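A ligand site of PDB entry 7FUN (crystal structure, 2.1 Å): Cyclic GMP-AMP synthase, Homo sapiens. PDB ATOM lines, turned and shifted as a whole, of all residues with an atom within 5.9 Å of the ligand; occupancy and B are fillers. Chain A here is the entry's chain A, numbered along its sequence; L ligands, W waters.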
ATOM      1  N   LEU A  49      33.703  23.229  -4.820  1.00  0.00           N
ATOM      2  CA  LEU A  49      33.217  21.947  -4.318  1.00  0.00           C
ATOM      3  C   LEU A  49      34.372  20.987  -4.076  1.00  0.00           C
ATOM      4  O   LEU A  49      34.592  20.577  -2.924  1.00  0.00           O
ATOM      5  CB  LEU A  49      32.127  21.342  -5.233  1.00  0.00           C
ATOM      6  CG  LEU A  49      31.647  19.894  -4.955  1.00  0.00           C
ATOM      7  CD1 LEU A  49      31.290  19.665  -3.504  1.00  0.00           C
ATOM      8  CD2 LEU A  49      30.449  19.553  -5.765  1.00  0.00           C
ATOM      9  N   ASN A  50      35.150  20.686  -5.139  1.00  0.00           N
ATOM     10  CA  ASN A  50      36.309  19.794  -5.078  1.00  0.00           C
ATOM     11  C   ASN A  50      37.606  20.542  -5.397  1.00  0.00           C
ATOM     12  O   ASN A  50      37.684  21.244  -6.406  1.00  0.00           O
ATOM     13  CB  ASN A  50      36.102  18.522  -5.945  1.00  0.00           C
ATOM     14  CG  ASN A  50      35.820  18.765  -7.419  1.00  0.00           C
ATOM     15  OD1 ASN A  50      36.725  19.089  -8.206  1.00  0.00           O
ATOM     16  ND2 ASN A  50      34.571  18.573  -7.829  1.00  0.00           N
ATOM     17  N   GLU A  56      35.480  19.991 -13.572  1.00  0.00           N
ATOM     18  CA  GLU A  56      34.422  19.150 -14.188  1.00  0.00           C
ATOM     19  C   GLU A  56      34.034  19.613 -15.619  1.00  0.00           C
ATOM     20  O   GLU A  56      34.328  20.745 -16.009  1.00  0.00           O
ATOM     21  CB  GLU A  56      33.186  19.050 -13.273  1.00  0.00           C
ATOM     22  CG  GLU A  56      33.491  18.608 -11.844  1.00  0.00           C
ATOM     23  CD  GLU A  56      33.620  17.113 -11.611  1.00  0.00           C
ATOM     24  OE1 GLU A  56      32.605  16.390 -11.744  1.00  0.00           O
ATOM     25  OE2 GLU A  56      34.731  16.670 -11.251  1.00  0.00           O
ATOM     26  N   VAL A  58      30.645  19.156 -18.617  1.00  0.00           N
ATOM     27  CA  VAL A  58      29.287  18.684 -18.935  1.00  0.00           C
ATOM     28  C   VAL A  58      29.351  17.847 -20.228  1.00  0.00           C
ATOM     29  O   VAL A  58      28.973  16.669 -20.216  1.00  0.00           O
ATOM     30  CB  VAL A  58      28.199  19.804 -18.952  1.00  0.00           C
ATOM     31  CG1 VAL A  58      26.954  19.388 -19.732  1.00  0.00           C
ATOM     32  CG2 VAL A  58      27.830  20.226 -17.546  1.00  0.00           C
ATOM     33  N   ASP A  67      33.017  23.231 -16.208  1.00  0.00           N
ATOM     34  CA  ASP A  67      31.855  23.314 -15.310  1.00  0.00           C
ATOM     35  C   ASP A  67      32.332  23.329 -13.837  1.00  0.00           C
ATOM     36  O   ASP A  67      33.001  22.408 -13.405  1.00  0.00           O
ATOM     37  CB  ASP A  67      30.969  22.094 -15.632  1.00  0.00           C
ATOM     38  CG  ASP A  67      29.688  21.929 -14.873  1.00  0.00           C
ATOM     39  OD1 ASP A  67      29.003  22.946 -14.618  1.00  0.00           O
ATOM     40  OD2 ASP A  67      29.339  20.756 -14.567  1.00  0.00           O
ATOM     41  N   VAL A  68      32.121  24.464 -13.116  1.00  0.00           N
ATOM     42  CA  VAL A  68      32.609  24.602 -11.731  1.00  0.00           C
ATOM     43  C   VAL A  68      31.514  25.005 -10.741  1.00  0.00           C
ATOM     44  O   VAL A  68      30.555  25.732 -11.072  1.00  0.00           O
ATOM     45  CB  VAL A  68      33.875  25.514 -11.538  1.00  0.00           C
ATOM     46  CG1 VAL A  68      35.035  25.108 -12.442  1.00  0.00           C
ATOM     47  CG2 VAL A  68      33.576  26.986 -11.669  1.00  0.00           C
ATOM     48  N   MET A  69      31.686  24.552  -9.495  1.00  0.00           N
ATOM     49  CA  MET A  69      30.752  24.936  -8.445  1.00  0.00           C
ATOM     50  C   MET A  69      31.471  25.641  -7.307  1.00  0.00           C
ATOM     51  O   MET A  69      32.520  25.191  -6.833  1.00  0.00           O
ATOM     52  CB  MET A  69      29.948  23.750  -7.905  1.00  0.00           C
ATOM     53  CG  MET A  69      28.989  24.149  -6.797  1.00  0.00           C
ATOM     54  SD  MET A  69      28.652  22.817  -5.634  1.00  0.00           S
ATOM     55  CE  MET A  69      27.326  22.001  -6.476  1.00  0.00           C
ATOM     56  N   ASP A 159      31.259  27.293 -17.015  1.00  0.00           N
ATOM     57  CA  ASP A 159      29.988  27.458 -16.298  1.00  0.00           C
ATOM     58  C   ASP A 159      30.268  27.547 -14.796  1.00  0.00           C
ATOM     59  O   ASP A 159      30.984  26.728 -14.244  1.00  0.00           O
ATOM     60  CB  ASP A 159      29.013  26.286 -16.573  1.00  0.00           C
ATOM     61  CG  ASP A 159      28.240  26.321 -17.881  1.00  0.00           C
ATOM     62  OD1 ASP A 159      28.439  27.276 -18.671  1.00  0.00           O
ATOM     63  OD2 ASP A 159      27.429  25.399 -18.117  1.00  0.00           O
ATOM     64  N   THR A 161      28.377  27.708 -11.158  1.00  0.00           N
ATOM     65  CA  THR A 161      27.173  27.468 -10.373  1.00  0.00           C
ATOM     66  C   THR A 161      27.508  27.842  -8.934  1.00  0.00           C
ATOM     67  O   THR A 161      28.550  27.463  -8.416  1.00  0.00           O
ATOM     68  CB  THR A 161      26.757  25.971 -10.498  1.00  0.00           C
ATOM     69  OG1 THR A 161      26.345  25.706 -11.820  1.00  0.00           O
ATOM     70  CG2 THR A 161      25.633  25.589  -9.561  1.00  0.00           C
ATOM     71  N   LEU A 178      17.957   6.917  -5.080  1.00  0.00           N
ATOM     72  CA  LEU A 178      19.251   6.203  -5.081  1.00  0.00           C
ATOM     73  C   LEU A 178      19.011   4.696  -4.869  1.00  0.00           C
ATOM     74  O   LEU A 178      19.560   4.090  -3.966  1.00  0.00           O
ATOM     75  CB  LEU A 178      20.198   6.830  -4.049  1.00  0.00           C
ATOM     76  CG  LEU A 178      21.682   6.426  -4.035  1.00  0.00           C
ATOM     77  CD1 LEU A 178      22.380   6.835  -5.325  1.00  0.00           C
ATOM     78  CD2 LEU A 178      22.382   7.029  -2.804  1.00  0.00           C
ATOM     79  N   ILE A 180      19.954   1.755  -5.311  1.00  0.00           N
ATOM     80  CA  ILE A 180      21.177   1.007  -5.606  1.00  0.00           C
ATOM     81  C   ILE A 180      21.401  -0.246  -4.714  1.00  0.00           C
ATOM     82  O   ILE A 180      22.376  -0.942  -4.933  1.00  0.00           O
ATOM     83  CB  ILE A 180      22.395   1.996  -5.522  1.00  0.00           C
ATOM     84  CG1 ILE A 180      22.729   2.381  -4.047  1.00  0.00           C
ATOM     85  CG2 ILE A 180      22.172   3.242  -6.406  1.00  0.00           C
ATOM     86  CD1 ILE A 180      24.125   3.023  -3.801  1.00  0.00           C
ATOM     87  N   TRP A 183      22.411  -3.487  -6.392  1.00  0.00           N
ATOM     88  CA  TRP A 183      23.575  -3.346  -7.270  1.00  0.00           C
ATOM     89  C   TRP A 183      24.847  -3.040  -6.453  1.00  0.00           C
ATOM     90  O   TRP A 183      25.776  -3.865  -6.411  1.00  0.00           O
ATOM     91  CB  TRP A 183      23.236  -2.308  -8.366  1.00  0.00           C
ATOM     92  CG  TRP A 183      24.416  -1.649  -9.062  1.00  0.00           C
ATOM     93  CD1 TRP A 183      25.570  -2.250  -9.470  1.00  0.00           C
ATOM     94  CD2 TRP A 183      24.487  -0.282  -9.496  1.00  0.00           C
ATOM     95  NE1 TRP A 183      26.386  -1.325 -10.087  1.00  0.00           N
ATOM     96  CE2 TRP A 183      25.735  -0.123 -10.148  1.00  0.00           C
ATOM     97  CE3 TRP A 183      23.633   0.837  -9.378  1.00  0.00           C
ATOM     98  CZ2 TRP A 183      26.157   1.123 -10.649  1.00  0.00           C
ATOM     99  CZ3 TRP A 183      24.048   2.037  -9.900  1.00  0.00           C
ATOM    100  CH2 TRP A 183      25.307   2.187 -10.510  1.00  0.00           C
ATOM    101  N   ARG A 216      16.715  24.277  -6.133  1.00  0.00           N
ATOM    102  CA  ARG A 216      16.587  22.868  -6.506  1.00  0.00           C
ATOM    103  C   ARG A 216      17.593  22.018  -5.726  1.00  0.00           C
ATOM    104  O   ARG A 216      18.748  22.431  -5.573  1.00  0.00           O
ATOM    105  CB  ARG A 216      16.766  22.700  -8.029  1.00  0.00           C
ATOM    106  CG  ARG A 216      16.402  21.268  -8.504  1.00  0.00           C
ATOM    107  CD  ARG A 216      16.789  20.929  -9.927  1.00  0.00           C
ATOM    108  NE  ARG A 216      18.185  21.263 -10.245  1.00  0.00           N
ATOM    109  CZ  ARG A 216      19.231  20.449 -10.081  1.00  0.00           C
ATOM    110  NH1 ARG A 216      19.081  19.246  -9.537  1.00  0.00           N
ATOM    111  NH2 ARG A 216      20.446  20.857 -10.426  1.00  0.00           N
ATOM    112  N   LEU A 217      17.180  20.802  -5.269  1.00  0.00           N
ATOM    113  CA  LEU A 217      18.113  19.880  -4.593  1.00  0.00           C
ATOM    114  C   LEU A 217      19.045  19.272  -5.663  1.00  0.00           C
ATOM    115  O   LEU A 217      18.562  18.763  -6.679  1.00  0.00           O
ATOM    116  CB  LEU A 217      17.424  18.695  -3.900  1.00  0.00           C
ATOM    117  CG  LEU A 217      16.355  18.897  -2.867  1.00  0.00           C
ATOM    118  CD1 LEU A 217      15.799  17.549  -2.426  1.00  0.00           C
ATOM    119  CD2 LEU A 217      16.894  19.650  -1.635  1.00  0.00           C
ATOM    120  N   SER A 218      20.365  19.309  -5.392  1.00  0.00           N
ATOM    121  CA  SER A 218      21.409  18.760  -6.250  1.00  0.00           C
ATOM    122  C   SER A 218      22.243  17.685  -5.539  1.00  0.00           C
ATOM    123  O   SER A 218      22.705  17.902  -4.410  1.00  0.00           O
ATOM    124  CB  SER A 218      22.325  19.866  -6.751  1.00  0.00           C
ATOM    125  OG  SER A 218      23.264  19.317  -7.647  1.00  0.00           O
ATOM    126  N   PHE A 219      22.438  16.537  -6.203  1.00  0.00           N
ATOM    127  CA  PHE A 219      23.248  15.409  -5.722  1.00  0.00           C
ATOM    128  C   PHE A 219      24.293  15.073  -6.788  1.00  0.00           C
ATOM    129  O   PHE A 219      24.753  13.941  -6.831  1.00  0.00           O
ATOM    130  CB  PHE A 219      22.353  14.188  -5.434  1.00  0.00           C
ATOM    131  CG  PHE A 219      21.290  14.442  -4.387  1.00  0.00           C
ATOM    132  CD1 PHE A 219      21.574  14.311  -3.033  1.00  0.00           C
ATOM    133  CD2 PHE A 219      20.008  14.847  -4.761  1.00  0.00           C
ATOM    134  CE1 PHE A 219      20.603  14.576  -2.066  1.00  0.00           C
ATOM    135  CE2 PHE A 219      19.038  15.135  -3.790  1.00  0.00           C
ATOM    136  CZ  PHE A 219      19.340  14.995  -2.447  1.00  0.00           C
ATOM    137  N   SER A 220      24.677  16.072  -7.628  1.00  0.00           N
ATOM    138  CA  SER A 220      25.614  15.860  -8.727  1.00  0.00           C
ATOM    139  C   SER A 220      26.954  15.294  -8.273  1.00  0.00           C
ATOM    140  O   SER A 220      27.567  14.517  -9.008  1.00  0.00           O
ATOM    141  CB  SER A 220      25.789  17.129  -9.562  1.00  0.00           C
ATOM    142  OG  SER A 220      26.610  18.066  -8.915  1.00  0.00           O
ATOM    143  N   HIS A 221      27.367  15.633  -7.035  1.00  0.00           N
ATOM    144  CA  HIS A 221      28.625  15.171  -6.403  1.00  0.00           C
ATOM    145  C   HIS A 221      28.673  13.635  -6.156  1.00  0.00           C
ATOM    146  O   HIS A 221      29.752  13.110  -6.019  1.00  0.00           O
ATOM    147  CB  HIS A 221      28.873  15.939  -5.098  1.00  0.00           C
ATOM    148  CG  HIS A 221      27.776  15.733  -4.082  1.00  0.00           C
ATOM    149  ND1 HIS A 221      26.464  16.147  -4.337  1.00  0.00           N
ATOM    150  CD2 HIS A 221      27.843  15.222  -2.829  1.00  0.00           C
ATOM    151  CE1 HIS A 221      25.767  15.845  -3.248  1.00  0.00           C
ATOM    152  NE2 HIS A 221      26.545  15.273  -2.311  1.00  0.00           N
ATOM    153  N   ILE A 222      27.522  12.950  -6.109  1.00  0.00           N
ATOM    154  CA  ILE A 222      27.407  11.491  -5.864  1.00  0.00           C
ATOM    155  C   ILE A 222      27.836  10.675  -7.076  1.00  0.00           C
ATOM    156  O   ILE A 222      28.271   9.545  -6.905  1.00  0.00           O
ATOM    157  CB  ILE A 222      25.947  11.135  -5.392  1.00  0.00           C
ATOM    158  CG1 ILE A 222      25.516  12.012  -4.157  1.00  0.00           C
ATOM    159  CG2 ILE A 222      25.778   9.597  -5.106  1.00  0.00           C
ATOM    160  CD1 ILE A 222      26.441  11.894  -2.888  1.00  0.00           C
ATOM    161  N   GLU A 223      27.742  11.257  -8.280  1.00  0.00           N
ATOM    162  CA  GLU A 223      28.109  10.580  -9.509  1.00  0.00           C
ATOM    163  C   GLU A 223      29.535  10.006  -9.537  1.00  0.00           C
ATOM    164  O   GLU A 223      29.694   8.863  -9.954  1.00  0.00           O
ATOM    165  CB  GLU A 223      27.902  11.504 -10.715  1.00  0.00           C
ATOM    166  CG  GLU A 223      28.116  10.798 -12.046  1.00  0.00           C
ATOM    167  CD  GLU A 223      28.073  11.620 -13.320  1.00  0.00           C
ATOM    168  OE1 GLU A 223      27.857  12.852 -13.233  1.00  0.00           O
ATOM    169  OE2 GLU A 223      28.221  11.019 -14.410  1.00  0.00           O
ATOM    170  N   ILE A 226      30.083   6.900  -7.357  1.00  0.00           N
ATOM    171  CA  ILE A 226      29.577   5.677  -7.918  1.00  0.00           C
ATOM    172  C   ILE A 226      30.400   5.296  -9.145  1.00  0.00           C
ATOM    173  O   ILE A 226      30.793   4.142  -9.241  1.00  0.00           O
ATOM    174  CB  ILE A 226      28.058   5.762  -8.172  1.00  0.00           C
ATOM    175  CG1 ILE A 226      27.329   5.641  -6.804  1.00  0.00           C
ATOM    176  CG2 ILE A 226      27.583   4.687  -9.207  1.00  0.00           C
ATOM    177  CD1 ILE A 226      25.930   6.075  -6.815  1.00  0.00           C
ATOM    178  N   SER A 275      22.955  16.279 -20.890  1.00  0.00           N
ATOM    179  CA  SER A 275      23.660  15.076 -20.480  1.00  0.00           C
ATOM    180  C   SER A 275      23.106  14.538 -19.146  1.00  0.00           C
ATOM    181  O   SER A 275      23.112  13.345 -18.943  1.00  0.00           O
ATOM    182  CB  SER A 275      25.171  15.329 -20.411  1.00  0.00           C
ATOM    183  OG  SER A 275      25.433  16.341 -19.464  1.00  0.00           O
ATOM    184  N   TYR A 276      22.502  15.421 -18.316  1.00  0.00           N
ATOM    185  CA  TYR A 276      21.839  15.079 -17.061  1.00  0.00           C
ATOM    186  C   TYR A 276      20.757  14.023 -17.322  1.00  0.00           C
ATOM    187  O   TYR A 276      20.702  13.029 -16.611  1.00  0.00           O
ATOM    188  CB  TYR A 276      21.260  16.337 -16.410  1.00  0.00           C
ATOM    189  CG  TYR A 276      20.406  16.083 -15.180  1.00  0.00           C
ATOM    190  CD1 TYR A 276      20.879  15.305 -14.121  1.00  0.00           C
ATOM    191  CD2 TYR A 276      19.132  16.651 -15.053  1.00  0.00           C
ATOM    192  CE1 TYR A 276      20.106  15.081 -12.978  1.00  0.00           C
ATOM    193  CE2 TYR A 276      18.376  16.473 -13.891  1.00  0.00           C
ATOM    194  CZ  TYR A 276      18.864  15.692 -12.851  1.00  0.00           C
ATOM    195  OH  TYR A 276      18.092  15.443 -11.741  1.00  0.00           O
ATOM    196  N   LYS A 279      22.454  10.714 -18.226  1.00  0.00           N
ATOM    197  CA  LYS A 279      23.050  10.145 -17.008  1.00  0.00           C
ATOM    198  C   LYS A 279      22.026   9.465 -16.160  1.00  0.00           C
ATOM    199  O   LYS A 279      22.227   8.312 -15.780  1.00  0.00           O
ATOM    200  CB  LYS A 279      23.757  11.234 -16.188  1.00  0.00           C
ATOM    201  CG  LYS A 279      24.935  11.843 -16.884  1.00  0.00           C
ATOM    202  CD  LYS A 279      25.789  12.577 -15.900  1.00  0.00           C
ATOM    203  CE  LYS A 279      25.622  14.071 -15.930  1.00  0.00           C
ATOM    204  NZ  LYS A 279      26.766  14.729 -15.245  1.00  0.00           N
ATOM    205  N   THR A 280      20.894  10.157 -15.868  1.00  0.00           N
ATOM    206  CA  THR A 280      19.752   9.659 -15.094  1.00  0.00           C
ATOM    207  C   THR A 280      19.247   8.327 -15.714  1.00  0.00           C
ATOM    208  O   THR A 280      19.163   7.335 -14.995  1.00  0.00           O
ATOM    209  CB  THR A 280      18.656  10.729 -15.057  1.00  0.00           C
ATOM    210  OG1 THR A 280      19.190  11.923 -14.500  1.00  0.00           O
ATOM    211  CG2 THR A 280      17.464  10.329 -14.246  1.00  0.00           C
ATOM    212  N   PHE A 283      21.875   5.481 -15.283  1.00  0.00           N
ATOM    213  CA  PHE A 283      21.887   4.949 -13.930  1.00  0.00           C
ATOM    214  C   PHE A 283      20.651   4.123 -13.610  1.00  0.00           C
ATOM    215  O   PHE A 283      20.764   3.184 -12.820  1.00  0.00           O
ATOM    216  CB  PHE A 283      22.152   6.026 -12.866  1.00  0.00           C
ATOM    217  CG  PHE A 283      23.610   6.449 -12.859  1.00  0.00           C
ATOM    218  CD1 PHE A 283      24.608   5.577 -12.444  1.00  0.00           C
ATOM    219  CD2 PHE A 283      23.988   7.725 -13.299  1.00  0.00           C
ATOM    220  CE1 PHE A 283      25.957   5.949 -12.487  1.00  0.00           C
ATOM    221  CE2 PHE A 283      25.338   8.117 -13.301  1.00  0.00           C
ATOM    222  CZ  PHE A 283      26.311   7.222 -12.899  1.00  0.00           C
ATOM    223  N   ASN A 322      13.862  11.479 -11.595  1.00  0.00           N
ATOM    224  CA  ASN A 322      15.074  11.970 -10.980  1.00  0.00           C
ATOM    225  C   ASN A 322      15.560  10.759 -10.160  1.00  0.00           C
ATOM    226  O   ASN A 322      14.748  10.120  -9.488  1.00  0.00           O
ATOM    227  CB  ASN A 322      14.725  13.178 -10.090  1.00  0.00           C
ATOM    228  CG  ASN A 322      15.845  13.773  -9.293  1.00  0.00           C
ATOM    229  OD1 ASN A 322      16.559  13.099  -8.575  1.00  0.00           O
ATOM    230  ND2 ASN A 322      15.985  15.079  -9.354  1.00  0.00           N
ATOM    231  N   TYR A 323      16.841  10.365 -10.321  1.00  0.00           N
ATOM    232  CA  TYR A 323      17.454   9.194  -9.683  1.00  0.00           C
ATOM    233  C   TYR A 323      17.380   9.250  -8.144  1.00  0.00           C
ATOM    234  O   TYR A 323      17.362   8.208  -7.481  1.00  0.00           O
ATOM    235  CB  TYR A 323      18.934   9.067 -10.137  1.00  0.00           C
ATOM    236  CG  TYR A 323      19.465   7.649 -10.034  1.00  0.00           C
ATOM    237  CD1 TYR A 323      18.975   6.645 -10.867  1.00  0.00           C
ATOM    238  CD2 TYR A 323      20.395   7.304  -9.060  1.00  0.00           C
ATOM    239  CE1 TYR A 323      19.356   5.316 -10.683  1.00  0.00           C
ATOM    240  CE2 TYR A 323      20.803   5.980  -8.891  1.00  0.00           C
ATOM    241  CZ  TYR A 323      20.313   5.004  -9.728  1.00  0.00           C
ATOM    242  OH  TYR A 323      20.795   3.728  -9.631  1.00  0.00           O
ATOM    243  N   PHE A 324      17.272  10.484  -7.591  1.00  0.00           N
ATOM    244  CA  PHE A 324      17.259  10.782  -6.163  1.00  0.00           C
ATOM    245  C   PHE A 324      15.889  11.104  -5.596  1.00  0.00           C
ATOM    246  O   PHE A 324      15.661  10.905  -4.401  1.00  0.00           O
ATOM    247  CB  PHE A 324      18.241  11.945  -5.897  1.00  0.00           C
ATOM    248  CG  PHE A 324      19.690  11.506  -6.084  1.00  0.00           C
ATOM    249  CD1 PHE A 324      20.278  11.519  -7.346  1.00  0.00           C
ATOM    250  CD2 PHE A 324      20.447  11.081  -5.013  1.00  0.00           C
ATOM    251  CE1 PHE A 324      21.568  11.034  -7.541  1.00  0.00           C
ATOM    252  CE2 PHE A 324      21.765  10.663  -5.188  1.00  0.00           C
ATOM    253  CZ  PHE A 324      22.319  10.639  -6.458  1.00  0.00           C
HETATM  254  C1  LIG L   1      30.281  21.723 -11.402  1.00  0.00           C
HETATM  255  C2  LIG L   1      31.410  21.249 -10.746  1.00  0.00           C
HETATM  256  C3  LIG L   1      30.017  20.346  -9.023  1.00  0.00           C
HETATM  257  C4  LIG L   1      24.019  17.169 -13.259  1.00  0.00           C
HETATM  258  C5  LIG L   1      23.158  16.057 -11.574  1.00  0.00           C
HETATM  259  C6  LIG L   1      23.995  15.222 -12.319  1.00  0.00           C
HETATM  260  C7  LIG L   1      24.171  13.886 -11.973  1.00  0.00           C
HETATM  261  C8  LIG L   1      23.506  13.367 -10.855  1.00  0.00           C
HETATM  262  C9  LIG L   1      23.624  11.923 -10.514  1.00  0.00           C
HETATM  263  C10 LIG L   1      22.833  10.927 -11.124  1.00  0.00           C
HETATM  264  C11 LIG L   1      22.937   9.592 -10.772  1.00  0.00           C
HETATM  265  C12 LIG L   1      23.831   9.200  -9.774  1.00  0.00           C
HETATM  266  C13 LIG L   1      23.963   7.742  -9.383  1.00  0.00           C
HETATM  267  C14 LIG L   1      24.611  10.174  -9.165  1.00  0.00           C
HETATM  268  C15 LIG L   1      24.357  18.327 -14.132  1.00  0.00           C
HETATM  269  C16 LIG L   1      31.279  20.565  -9.554  1.00  0.00           C
HETATM  270  C17 LIG L   1      28.888  20.834  -9.681  1.00  0.00           C
HETATM  271  C18 LIG L   1      24.508  11.518  -9.511  1.00  0.00           C
HETATM  272  C19 LIG L   1      25.409  20.516 -14.192  1.00  0.00           C
HETATM  273  C20 LIG L   1      22.631  14.191 -10.134  1.00  0.00           C
HETATM  274  C21 LIG L   1      22.501  15.556 -10.431  1.00  0.00           C
HETATM  275  C22 LIG L   1      21.591  16.405  -9.578  1.00  0.00           C
HETATM  276  C23 LIG L   1      26.056  21.567 -13.283  1.00  0.00           C
HETATM  277  C24 LIG L   1      27.142  19.691 -12.085  1.00  0.00           C
HETATM  278  C25 LIG L   1      26.489  18.758 -13.068  1.00  0.00           C
HETATM  279  C26 LIG L   1      27.780  22.000 -11.625  1.00  0.00           C
HETATM  280  C27 LIG L   1      29.007  21.525 -10.878  1.00  0.00           C
HETATM  281  N1  LIG L   1      23.273  17.307 -12.137  1.00  0.00           N
HETATM  282  N2  LIG L   1      24.514  15.954 -13.389  1.00  0.00           N
HETATM  283  N3  LIG L   1      25.181  19.292 -13.438  1.00  0.00           N
HETATM  284  N4  LIG L   1      27.310  21.061 -12.658  1.00  0.00           N
HETATM  285  O1  LIG L   1      21.481  17.617  -9.895  1.00  0.00           O
HETATM  286  O2  LIG L   1      20.984  15.864  -8.621  1.00  0.00           O
HETATM  287 CL1  LIG L   1      21.730  11.352 -12.395  1.00  0.00          CL
HETATM  288  O   HOH W   1      18.156  16.401  -7.989  1.00  0.00           O
HETATM  289  O   HOH W   2      18.501  12.272 -11.609  1.00  0.00           O
HETATM  290  O   HOH W   3      20.850  19.499 -13.066  1.00  0.00           O
HETATM  291  O   HOH W   4      19.155  14.003  -9.508  1.00  0.00           O
HETATM  292  O   HOH W   5      29.269  17.385  -9.087  1.00  0.00           O
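The backbone NH of Phe 219 is in hydrogen-bond range of an oxygen (O2) of the ligand.
A nitrogen (N4) of the ligand lies within salt-bridge range of the side-chain carboxylate of Asp 67 (2.8 Å).
An oxygen (O1) of the ligand lies within salt-bridge range of the guanidinium group (NH1) of Arg 216, 2.9 Å away.
The side-chain hydroxyl (OG) of Ser 218 is in hydrogen-bond range of an oxygen (O1) of the ligand (3.3 Å).
NZ of Lys 279 is in hydrogen-bond range of N2 of the ligand (3.2 Å).
The backbone NH (N) of Asp 67 lies within hydrogen-bond range of the backbone carbonyl oxygen (O) of Glu 56 (2.8 Å).
The backbone NH (N) of Phe 324 lies within hydrogen-bond range of the side-chain amide oxygen (OD1) of Asn 322.
OH of Tyr 323 is in hydrogen-bond range of O of Phe 283, 3.2 Å away.
N of Leu 49 is in hydrogen-bond range of O of Met 69, 3.0 Å away.
The side-chain amide nitrogen (ND2) of Asn 322 is in hydrogen-bond range of the side-chain hydroxyl (OH) of Tyr 276.
The backbone NH (N) of Val 68 is in hydrogen-bond range of the backbone carbonyl oxygen (O) of Asp 159.
O of Val 68 lies within hydrogen-bond range of N of Thr 161.
OG1 of Thr 280 is in hydrogen-bond range of O of Tyr 276 (2.8 Å).
Residues that only touch the ligand: Phe 283 (3.3 Å), Thr 280 (3.3 Å), Leu 49 (3.4 Å), Glu 223 (3.4 Å), Ser 220 (3.5 Å), Tyr 276 (3.5 Å), Glu 56 (3.5 Å), Met 69 (3.5 Å), Phe 324 (3.6 Å), Val 68 (3.6 Å), Tyr 323 (3.6 Å), Ile 226 (3.6 Å), Ile 222 (3.9 Å) and Thr 161 (3.98 Å).
19 residues have an atom within 4 Å of the ligand: Leu 49, Glu 56, Asp 67, Val 68, Met 69, Thr 161, Arg 216, Ser 218, Phe 219, Ser 220, Ile 222, Glu 223, Ile 226, Tyr 276, Lys 279, Thr 280, Phe 283, Tyr 323 and Phe 324.
Water W4 lies within hydrogen-bond range of an oxygen (O2) of the ligand (2.8 Å), the side-chain hydroxyl of Tyr 276 (2.9 Å) and the side-chain amide oxygen of Asn 322 (2.9 Å).
Water W1 lies within hydrogen-bond range of the backbone carbonyl oxygen of Leu 217, the side-chain amide nitrogen of Asn 322, an oxygen (O2) of the ligand and the guanidinium group of Arg 216.
Water W5 lies within hydrogen-bond range of the side-chain hydroxyl (OG) of Ser 220 (2.8 Å) and the backbone NH (N) of His 221 (3.3 Å).
Water W3 bridges NH2 of Arg 216 (3.0 Å) and N1 of the ligand (3.4 Å).
Water W2 lies within hydrogen-bond range of N of Tyr 323 (2.8 Å), OG1 of Thr 280 (3.0 Å) and OH of Tyr 276 (3.2 Å).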
